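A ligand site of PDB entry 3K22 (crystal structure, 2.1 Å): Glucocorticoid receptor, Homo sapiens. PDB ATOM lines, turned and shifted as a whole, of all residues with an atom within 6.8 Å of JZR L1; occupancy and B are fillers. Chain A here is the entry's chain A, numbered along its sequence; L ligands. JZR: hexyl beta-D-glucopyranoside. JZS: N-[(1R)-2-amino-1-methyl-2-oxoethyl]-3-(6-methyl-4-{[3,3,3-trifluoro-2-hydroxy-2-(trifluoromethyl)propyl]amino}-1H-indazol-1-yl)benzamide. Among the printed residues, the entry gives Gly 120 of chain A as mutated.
An oxygen (O1) of JZR L1 sits close to the side-chain sulfur of Met 42, at 3.4 Å. Thr 38 touches JZR L1. Leu 45 touches JZR L1 (CD1 to C5', 3.9 Å). Pro 119 touches JZR L1. Met 121 touches JZR L1. Gln 124 touches JZR L1 (CB to C6', 3.7 Å). Met 128 touches JZR L1. Met 227 touches JZR L1. Hydrophobic or aromatic side chains that line JZR L1: Met 42, Leu 45, Pro 119, Met 121, Met 128, Tyr 217 and Met 227. The nearest printed residue that does not touch JZR L1 is Thr 221 (4.1 Å).
O2 of JZS L2 sits close to O of Leu 45 (3.1 Å). The backbone NH (N) of Gly 120 is in hydrogen-bond range of an oxygen (O6) of JZR L1, 3.1 Å away. The side-chain hydroxyl (OH) of Tyr 217 is in hydrogen-bond range of an oxygen (O1) of JZR L1, 2.9 Å away.
O of Met 121 is in hydrogen-bond range of SG of Cys 125 (3.3 Å). OG1 of Thr 221 sits at hydrogen-bond distance from O of Tyr 217, at 3.0 Å. The side-chain carboxylate (OD2) of Asp 224 lies within hydrogen-bond range of the backbone NH (N) of Met 227. The side-chain hydroxyl of Thr 38 is in hydrogen-bond range of the backbone carbonyl oxygen of Pro 119 (3.1 Å). The side-chain hydroxyl (OH) of Tyr 217 is in hydrogen-bond range of the side-chain sulfur (SD) of Met 42 (3.8 Å).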
ATOM      1  N   THR A  38      27.488 -17.321 -14.416  1.00  0.00           N
ATOM      2  CA  THR A  38      26.564 -16.187 -14.317  1.00  0.00           C
ATOM      3  C   THR A  38      26.474 -15.470 -15.663  1.00  0.00           C
ATOM      4  O   THR A  38      25.380 -15.237 -16.170  1.00  0.00           O
ATOM      5  CB  THR A  38      26.935 -15.202 -13.177  1.00  0.00           C
ATOM      6  OG1 THR A  38      26.966 -15.888 -11.917  1.00  0.00           O
ATOM      7  CG2 THR A  38      25.909 -14.066 -13.067  1.00  0.00           C
ATOM      8  N   TRP A  39      27.615 -15.132 -16.246  1.00  0.00           N
ATOM      9  CA  TRP A  39      27.647 -14.540 -17.586  1.00  0.00           C
ATOM     10  C   TRP A  39      26.810 -15.355 -18.565  1.00  0.00           C
ATOM     11  O   TRP A  39      26.017 -14.805 -19.332  1.00  0.00           O
ATOM     12  CB  TRP A  39      29.095 -14.428 -18.089  1.00  0.00           C
ATOM     13  CG  TRP A  39      29.225 -13.748 -19.416  1.00  0.00           C
ATOM     14  CD1 TRP A  39      29.402 -12.422 -19.644  1.00  0.00           C
ATOM     15  CD2 TRP A  39      29.176 -14.371 -20.713  1.00  0.00           C
ATOM     16  NE1 TRP A  39      29.468 -12.169 -20.992  1.00  0.00           N
ATOM     17  CE2 TRP A  39      29.324 -13.354 -21.670  1.00  0.00           C
ATOM     18  CE3 TRP A  39      29.014 -15.695 -21.147  1.00  0.00           C
ATOM     19  CZ2 TRP A  39      29.330 -13.614 -23.051  1.00  0.00           C
ATOM     20  CZ3 TRP A  39      29.015 -15.958 -22.518  1.00  0.00           C
ATOM     21  CH2 TRP A  39      29.173 -14.920 -23.454  1.00  0.00           C
ATOM     22  N   ILE A  41      24.338 -17.456 -17.967  1.00  0.00           N
ATOM     23  CA  ILE A  41      22.923 -17.318 -17.647  1.00  0.00           C
ATOM     24  C   ILE A  41      22.392 -15.919 -17.998  1.00  0.00           C
ATOM     25  O   ILE A  41      21.320 -15.801 -18.575  1.00  0.00           O
ATOM     26  CB  ILE A  41      22.663 -17.640 -16.157  1.00  0.00           C
ATOM     27  CG1 ILE A  41      22.887 -19.133 -15.914  1.00  0.00           C
ATOM     28  CG2 ILE A  41      21.250 -17.248 -15.761  1.00  0.00           C
ATOM     29  CD1 ILE A  41      22.893 -19.514 -14.459  1.00  0.00           C
ATOM     30  N   MET A  42      23.156 -14.886 -17.655  1.00  0.00           N
ATOM     31  CA  MET A  42      22.820 -13.517 -18.019  1.00  0.00           C
ATOM     32  C   MET A  42      22.503 -13.408 -19.512  1.00  0.00           C
ATOM     33  O   MET A  42      21.480 -12.850 -19.914  1.00  0.00           O
ATOM     34  CB  MET A  42      23.978 -12.557 -17.660  1.00  0.00           C
ATOM     35  CG  MET A  42      24.125 -12.257 -16.166  1.00  0.00           C
ATOM     36  SD  MET A  42      25.455 -11.068 -15.730  1.00  0.00           S
ATOM     37  CE  MET A  42      26.860 -12.120 -15.375  1.00  0.00           C
ATOM     38  N   LEU A  45      19.241 -15.359 -20.627  1.00  0.00           N
ATOM     39  CA  LEU A  45      18.013 -14.732 -20.134  1.00  0.00           C
ATOM     40  C   LEU A  45      17.686 -13.438 -20.880  1.00  0.00           C
ATOM     41  O   LEU A  45      16.519 -13.089 -21.033  1.00  0.00           O
ATOM     42  CB  LEU A  45      18.110 -14.462 -18.626  1.00  0.00           C
ATOM     43  CG  LEU A  45      18.077 -15.705 -17.731  1.00  0.00           C
ATOM     44  CD1 LEU A  45      18.453 -15.366 -16.294  1.00  0.00           C
ATOM     45  CD2 LEU A  45      16.706 -16.344 -17.794  1.00  0.00           C
ATOM     46  N   PHE A 105      12.546 -20.250 -15.332  1.00  0.00           N
ATOM     47  CA  PHE A 105      12.568 -19.419 -16.537  1.00  0.00           C
ATOM     48  C   PHE A 105      12.102 -20.183 -17.767  1.00  0.00           C
ATOM     49  O   PHE A 105      11.387 -19.635 -18.613  1.00  0.00           O
ATOM     50  CB  PHE A 105      13.962 -18.860 -16.771  1.00  0.00           C
ATOM     51  CG  PHE A 105      14.303 -17.728 -15.861  1.00  0.00           C
ATOM     52  CD1 PHE A 105      15.011 -17.937 -14.690  1.00  0.00           C
ATOM     53  CD2 PHE A 105      13.900 -16.437 -16.176  1.00  0.00           C
ATOM     54  CE1 PHE A 105      15.330 -16.878 -13.857  1.00  0.00           C
ATOM     55  CE2 PHE A 105      14.215 -15.369 -15.354  1.00  0.00           C
ATOM     56  CZ  PHE A 105      14.926 -15.592 -14.186  1.00  0.00           C
ATOM     57  N   LEU A 118      25.158 -18.811  -7.082  1.00  0.00           N
ATOM     58  CA  LEU A 118      26.098 -18.210  -8.039  1.00  0.00           C
ATOM     59  C   LEU A 118      26.189 -16.698  -7.796  1.00  0.00           C
ATOM     60  O   LEU A 118      25.229 -16.087  -7.325  1.00  0.00           O
ATOM     61  CB  LEU A 118      25.679 -18.474  -9.495  1.00  0.00           C
ATOM     62  CG  LEU A 118      25.989 -19.863 -10.056  1.00  0.00           C
ATOM     63  CD1 LEU A 118      25.238 -20.074 -11.372  1.00  0.00           C
ATOM     64  CD2 LEU A 118      27.495 -20.060 -10.251  1.00  0.00           C
ATOM     65  N   PRO A 119      27.341 -16.091  -8.135  1.00  0.00           N
ATOM     66  CA  PRO A 119      27.574 -14.692  -7.772  1.00  0.00           C
ATOM     67  C   PRO A 119      26.592 -13.731  -8.454  1.00  0.00           C
ATOM     68  O   PRO A 119      26.364 -13.844  -9.667  1.00  0.00           O
ATOM     69  CB  PRO A 119      29.009 -14.427  -8.234  1.00  0.00           C
ATOM     70  CG  PRO A 119      29.254 -15.436  -9.289  1.00  0.00           C
ATOM     71  CD  PRO A 119      28.478 -16.649  -8.885  1.00  0.00           C
ATOM     72  N   GLY A 120      26.020 -12.813  -7.674  1.00  0.00           N
ATOM     73  CA  GLY A 120      25.062 -11.829  -8.168  1.00  0.00           C
ATOM     74  C   GLY A 120      23.654 -12.354  -8.373  1.00  0.00           C
ATOM     75  O   GLY A 120      22.723 -11.559  -8.538  1.00  0.00           O
ATOM     76  N   MET A 121      23.475 -13.674  -8.337  1.00  0.00           N
ATOM     77  CA  MET A 121      22.213 -14.284  -8.728  1.00  0.00           C
ATOM     78  C   MET A 121      21.081 -13.932  -7.776  1.00  0.00           C
ATOM     79  O   MET A 121      20.043 -13.425  -8.211  1.00  0.00           O
ATOM     80  CB  MET A 121      22.353 -15.812  -8.771  1.00  0.00           C
ATOM     81  CG  MET A 121      21.255 -16.492  -9.553  1.00  0.00           C
ATOM     82  SD  MET A 121      21.358 -16.109 -11.310  1.00  0.00           S
ATOM     83  CE  MET A 121      22.999 -16.681 -11.739  1.00  0.00           C
ATOM     84  N   TYR A 122      21.284 -14.180  -6.490  1.00  0.00           N
ATOM     85  CA  TYR A 122      20.248 -13.925  -5.490  1.00  0.00           C
ATOM     86  C   TYR A 122      19.879 -12.452  -5.384  1.00  0.00           C
ATOM     87  O   TYR A 122      18.728 -12.134  -5.108  1.00  0.00           O
ATOM     88  CB  TYR A 122      20.633 -14.463  -4.107  1.00  0.00           C
ATOM     89  CG  TYR A 122      19.505 -14.256  -3.129  1.00  0.00           C
ATOM     90  CD1 TYR A 122      18.400 -15.098  -3.134  1.00  0.00           C
ATOM     91  CD2 TYR A 122      19.511 -13.192  -2.229  1.00  0.00           C
ATOM     92  CE1 TYR A 122      17.342 -14.899  -2.263  1.00  0.00           C
ATOM     93  CE2 TYR A 122      18.457 -12.985  -1.354  1.00  0.00           C
ATOM     94  CZ  TYR A 122      17.376 -13.849  -1.366  1.00  0.00           C
ATOM     95  OH  TYR A 122      16.325 -13.660  -0.507  1.00  0.00           O
ATOM     96  N   ASP A 123      20.847 -11.568  -5.585  1.00  0.00           N
ATOM     97  CA  ASP A 123      20.584 -10.133  -5.455  1.00  0.00           C
ATOM     98  C   ASP A 123      19.493  -9.679  -6.428  1.00  0.00           C
ATOM     99  O   ASP A 123      18.746  -8.754  -6.120  1.00  0.00           O
ATOM    100  CB  ASP A 123      21.858  -9.288  -5.634  1.00  0.00           C
ATOM    101  CG  ASP A 123      21.744  -7.885  -5.004  1.00  0.00           C
ATOM    102  OD1 ASP A 123      20.673  -7.541  -4.447  1.00  0.00           O
ATOM    103  OD2 ASP A 123      22.728  -7.122  -5.053  1.00  0.00           O
ATOM    104  N   GLN A 124      19.394 -10.326  -7.584  1.00  0.00           N
ATOM    105  CA  GLN A 124      18.354 -10.008  -8.553  1.00  0.00           C
ATOM    106  C   GLN A 124      17.148 -10.935  -8.436  1.00  0.00           C
ATOM    107  O   GLN A 124      16.007 -10.484  -8.547  1.00  0.00           O
ATOM    108  CB  GLN A 124      18.903 -10.064  -9.971  1.00  0.00           C
ATOM    109  CG  GLN A 124      20.101  -9.164 -10.190  1.00  0.00           C
ATOM    110  CD  GLN A 124      19.860  -7.743  -9.713  1.00  0.00           C
ATOM    111  OE1 GLN A 124      18.771  -7.197  -9.864  1.00  0.00           O
ATOM    112  NE2 GLN A 124      20.887  -7.134  -9.120  1.00  0.00           N
ATOM    113  N   CYS A 125      17.410 -12.224  -8.206  1.00  0.00           N
ATOM    114  CA  CYS A 125      16.329 -13.209  -8.164  1.00  0.00           C
ATOM    115  C   CYS A 125      15.381 -13.038  -6.991  1.00  0.00           C
ATOM    116  O   CYS A 125      14.239 -13.484  -7.065  1.00  0.00           O
ATOM    117  CB  CYS A 125      16.915 -14.611  -8.118  1.00  0.00           C
ATOM    118  SG  CYS A 125      17.636 -15.128  -9.654  1.00  0.00           S
ATOM    119  N   MET A 128      12.026 -11.561  -7.939  1.00  0.00           N
ATOM    120  CA  MET A 128      11.145 -12.436  -8.694  1.00  0.00           C
ATOM    121  C   MET A 128      10.620 -13.534  -7.770  1.00  0.00           C
ATOM    122  O   MET A 128       9.494 -14.004  -7.934  1.00  0.00           O
ATOM    123  CB  MET A 128      11.882 -13.029  -9.883  1.00  0.00           C
ATOM    124  CG  MET A 128      12.545 -11.979 -10.794  1.00  0.00           C
ATOM    125  SD  MET A 128      13.860 -12.656 -11.819  1.00  0.00           S
ATOM    126  CE  MET A 128      15.122 -11.382 -11.694  1.00  0.00           C
ATOM    127  N   LEU A 214      13.948  -4.599 -10.948  1.00  0.00           N
ATOM    128  CA  LEU A 214      14.383  -5.360 -12.116  1.00  0.00           C
ATOM    129  C   LEU A 214      14.839  -4.466 -13.269  1.00  0.00           C
ATOM    130  O   LEU A 214      15.830  -4.765 -13.938  1.00  0.00           O
ATOM    131  CB  LEU A 214      13.252  -6.273 -12.609  1.00  0.00           C
ATOM    132  CG  LEU A 214      12.790  -7.357 -11.640  1.00  0.00           C
ATOM    133  CD1 LEU A 214      11.557  -8.038 -12.165  1.00  0.00           C
ATOM    134  CD2 LEU A 214      13.903  -8.360 -11.389  1.00  0.00           C
ATOM    135  N   TYR A 217      18.313  -2.763 -12.599  1.00  0.00           N
ATOM    136  CA  TYR A 217      19.374  -3.716 -12.889  1.00  0.00           C
ATOM    137  C   TYR A 217      19.580  -3.873 -14.387  1.00  0.00           C
ATOM    138  O   TYR A 217      20.708  -3.785 -14.880  1.00  0.00           O
ATOM    139  CB  TYR A 217      19.066  -5.105 -12.295  1.00  0.00           C
ATOM    140  CG  TYR A 217      20.000  -6.155 -12.829  1.00  0.00           C
ATOM    141  CD1 TYR A 217      21.327  -6.215 -12.416  1.00  0.00           C
ATOM    142  CD2 TYR A 217      19.573  -7.077 -13.794  1.00  0.00           C
ATOM    143  CE1 TYR A 217      22.205  -7.175 -12.914  1.00  0.00           C
ATOM    144  CE2 TYR A 217      20.434  -8.046 -14.302  1.00  0.00           C
ATOM    145  CZ  TYR A 217      21.751  -8.077 -13.862  1.00  0.00           C
ATOM    146  OH  TYR A 217      22.605  -9.019 -14.365  1.00  0.00           O
ATOM    147  N   THR A 221      22.924  -2.810 -16.349  1.00  0.00           N
ATOM    148  CA  THR A 221      23.602  -3.826 -17.134  1.00  0.00           C
ATOM    149  C   THR A 221      23.763  -3.367 -18.582  1.00  0.00           C
ATOM    150  O   THR A 221      24.828  -3.525 -19.188  1.00  0.00           O
ATOM    151  CB  THR A 221      22.824  -5.167 -17.121  1.00  0.00           C
ATOM    152  OG1 THR A 221      22.788  -5.678 -15.781  1.00  0.00           O
ATOM    153  CG2 THR A 221      23.473  -6.190 -18.023  1.00  0.00           C
ATOM    154  N   ASP A 224      26.383  -0.477 -18.879  1.00  0.00           N
ATOM    155  CA  ASP A 224      27.722  -0.776 -18.395  1.00  0.00           C
ATOM    156  C   ASP A 224      28.601  -1.107 -19.601  1.00  0.00           C
ATOM    157  O   ASP A 224      28.331  -2.064 -20.325  1.00  0.00           O
ATOM    158  CB  ASP A 224      27.704  -1.930 -17.399  1.00  0.00           C
ATOM    159  CG  ASP A 224      29.059  -2.174 -16.756  1.00  0.00           C
ATOM    160  OD1 ASP A 224      29.909  -1.265 -16.741  1.00  0.00           O
ATOM    161  OD2 ASP A 224      29.259  -3.306 -16.257  1.00  0.00           O
ATOM    162  N   MET A 227      30.900  -4.129 -18.881  1.00  0.00           N
ATOM    163  CA  MET A 227      30.120  -5.364 -18.803  1.00  0.00           C
ATOM    164  C   MET A 227      30.251  -6.198 -20.072  1.00  0.00           C
ATOM    165  O   MET A 227      30.731  -7.325 -20.014  1.00  0.00           O
ATOM    166  CG  MET A 227      27.709  -6.406 -16.204  1.00  0.00           C
HETATM  167  C1  JZR L   1      25.534  -9.873 -12.014  1.00  0.00           C
HETATM  168  O1  JZR L   1      24.322 -10.453 -12.533  1.00  0.00           O
HETATM  169  C2  JZR L   1      25.837  -8.395 -12.254  1.00  0.00           C
HETATM  170  O2  JZR L   1      25.269  -7.939 -13.482  1.00  0.00           O
HETATM  171  C3  JZR L   1      27.337  -8.175 -12.316  1.00  0.00           C
HETATM  172  O3  JZR L   1      27.632  -6.784 -12.415  1.00  0.00           O
HETATM  173  C4  JZR L   1      27.944  -8.775 -11.056  1.00  0.00           C
HETATM  174  O4  JZR L   1      29.339  -8.444 -10.973  1.00  0.00           O
HETATM  175  C5  JZR L   1      27.738 -10.285 -11.066  1.00  0.00           C
HETATM  176  O5  JZR L   1      26.349 -10.624 -11.093  1.00  0.00           O
HETATM  177  C6  JZR L   1      28.394 -10.953  -9.851  1.00  0.00           C
HETATM  178  O6  JZR L   1      27.787 -10.503  -8.637  1.00  0.00           O
HETATM  179  C1' JZR L   1      23.650 -11.402 -11.698  1.00  0.00           C
HETATM  180  C2' JZR L   1      22.795 -12.357 -12.545  1.00  0.00           C
HETATM  181  C3' JZR L   1      21.479 -11.727 -13.021  1.00  0.00           C
HETATM  182  C4' JZR L   1      20.291 -12.673 -12.822  1.00  0.00           C
HETATM  183  C5' JZR L   1      19.156 -12.446 -13.826  1.00  0.00           C
HETATM  184  C6' JZR L   1      18.081 -11.510 -13.309  1.00  0.00           C
HETATM  185  C1  JZS L   2       3.581 -15.370 -20.638  1.00  0.00           C
HETATM  186  F1  JZS L   2      15.478 -10.084 -20.518  1.00  0.00           F
HETATM  187  N1  JZS L   2       5.963 -15.011 -20.401  1.00  0.00           N
HETATM  188  O1  JZS L   2       7.058 -13.047 -19.951  1.00  0.00           O
HETATM  189  C2  JZS L   2       4.699 -14.378 -20.661  1.00  0.00           C
HETATM  190  F2  JZS L   2      17.122  -8.677 -20.501  1.00  0.00           F
HETATM  191  N2  JZS L   2      11.635 -14.652 -18.726  1.00  0.00           N
HETATM  192  O2  JZS L   2      17.628 -10.983 -19.060  1.00  0.00           O
HETATM  193  C3  JZS L   2       6.993 -14.261 -19.924  1.00  0.00           C
HETATM  194  F3  JZS L   2      15.363  -8.269 -19.312  1.00  0.00           F
HETATM  195  N3  JZS L   2      12.468 -14.960 -19.718  1.00  0.00           N
HETATM  196  O3  JZS L   2       3.973 -13.069 -22.509  1.00  0.00           O
HETATM  197  C4  JZS L   2       8.083 -15.014 -19.335  1.00  0.00           C
HETATM  198  F4  JZS L   2      18.273  -8.199 -18.564  1.00  0.00           F
HETATM  199  N4  JZS L   2      15.272 -11.840 -18.412  1.00  0.00           N
HETATM  200  C5  JZS L   2       7.848 -16.264 -18.838  1.00  0.00           C
HETATM  201  F5  JZS L   2      18.471  -9.676 -17.012  1.00  0.00           F
HETATM  202  N5  JZS L   2       5.869 -14.330 -22.713  1.00  0.00           N
HETATM  203  C6  JZS L   2       8.890 -16.971 -18.280  1.00  0.00           C
HETATM  204  F6  JZS L   2      16.817  -8.271 -16.976  1.00  0.00           F
HETATM  205  C7  JZS L   2      10.149 -16.428 -18.249  1.00  0.00           C
HETATM  206  C8  JZS L   2      10.356 -15.170 -18.757  1.00  0.00           C
HETATM  207  C9  JZS L   2       9.335 -14.450 -19.313  1.00  0.00           C
HETATM  208  C10 JZS L   2      13.484 -14.108 -19.568  1.00  0.00           C
HETATM  209  C11 JZS L   2      13.299 -13.263 -18.467  1.00  0.00           C
HETATM  210  C12 JZS L   2      14.036 -12.248 -17.903  1.00  0.00           C
HETATM  211  C13 JZS L   2      15.695 -10.636 -17.739  1.00  0.00           C
HETATM  212  C14 JZS L   2      16.772  -9.978 -18.573  1.00  0.00           C
HETATM  213  C15 JZS L   2      16.178  -9.244 -19.740  1.00  0.00           C
HETATM  214  C16 JZS L   2      17.584  -9.026 -17.768  1.00  0.00           C
HETATM  215  C17 JZS L   2      13.476 -11.662 -16.797  1.00  0.00           C
HETATM  216  C18 JZS L   2      12.274 -12.055 -16.281  1.00  0.00           C
HETATM  217  C19 JZS L   2      11.742 -11.367 -15.087  1.00  0.00           C
HETATM  218  C20 JZS L   2      11.529 -13.060 -16.833  1.00  0.00           C
HETATM  219  C21 JZS L   2      12.093 -13.638 -17.935  1.00  0.00           C
HETATM  220  C22 JZS L   2       4.788 -13.845 -22.050  1.00  0.00           C
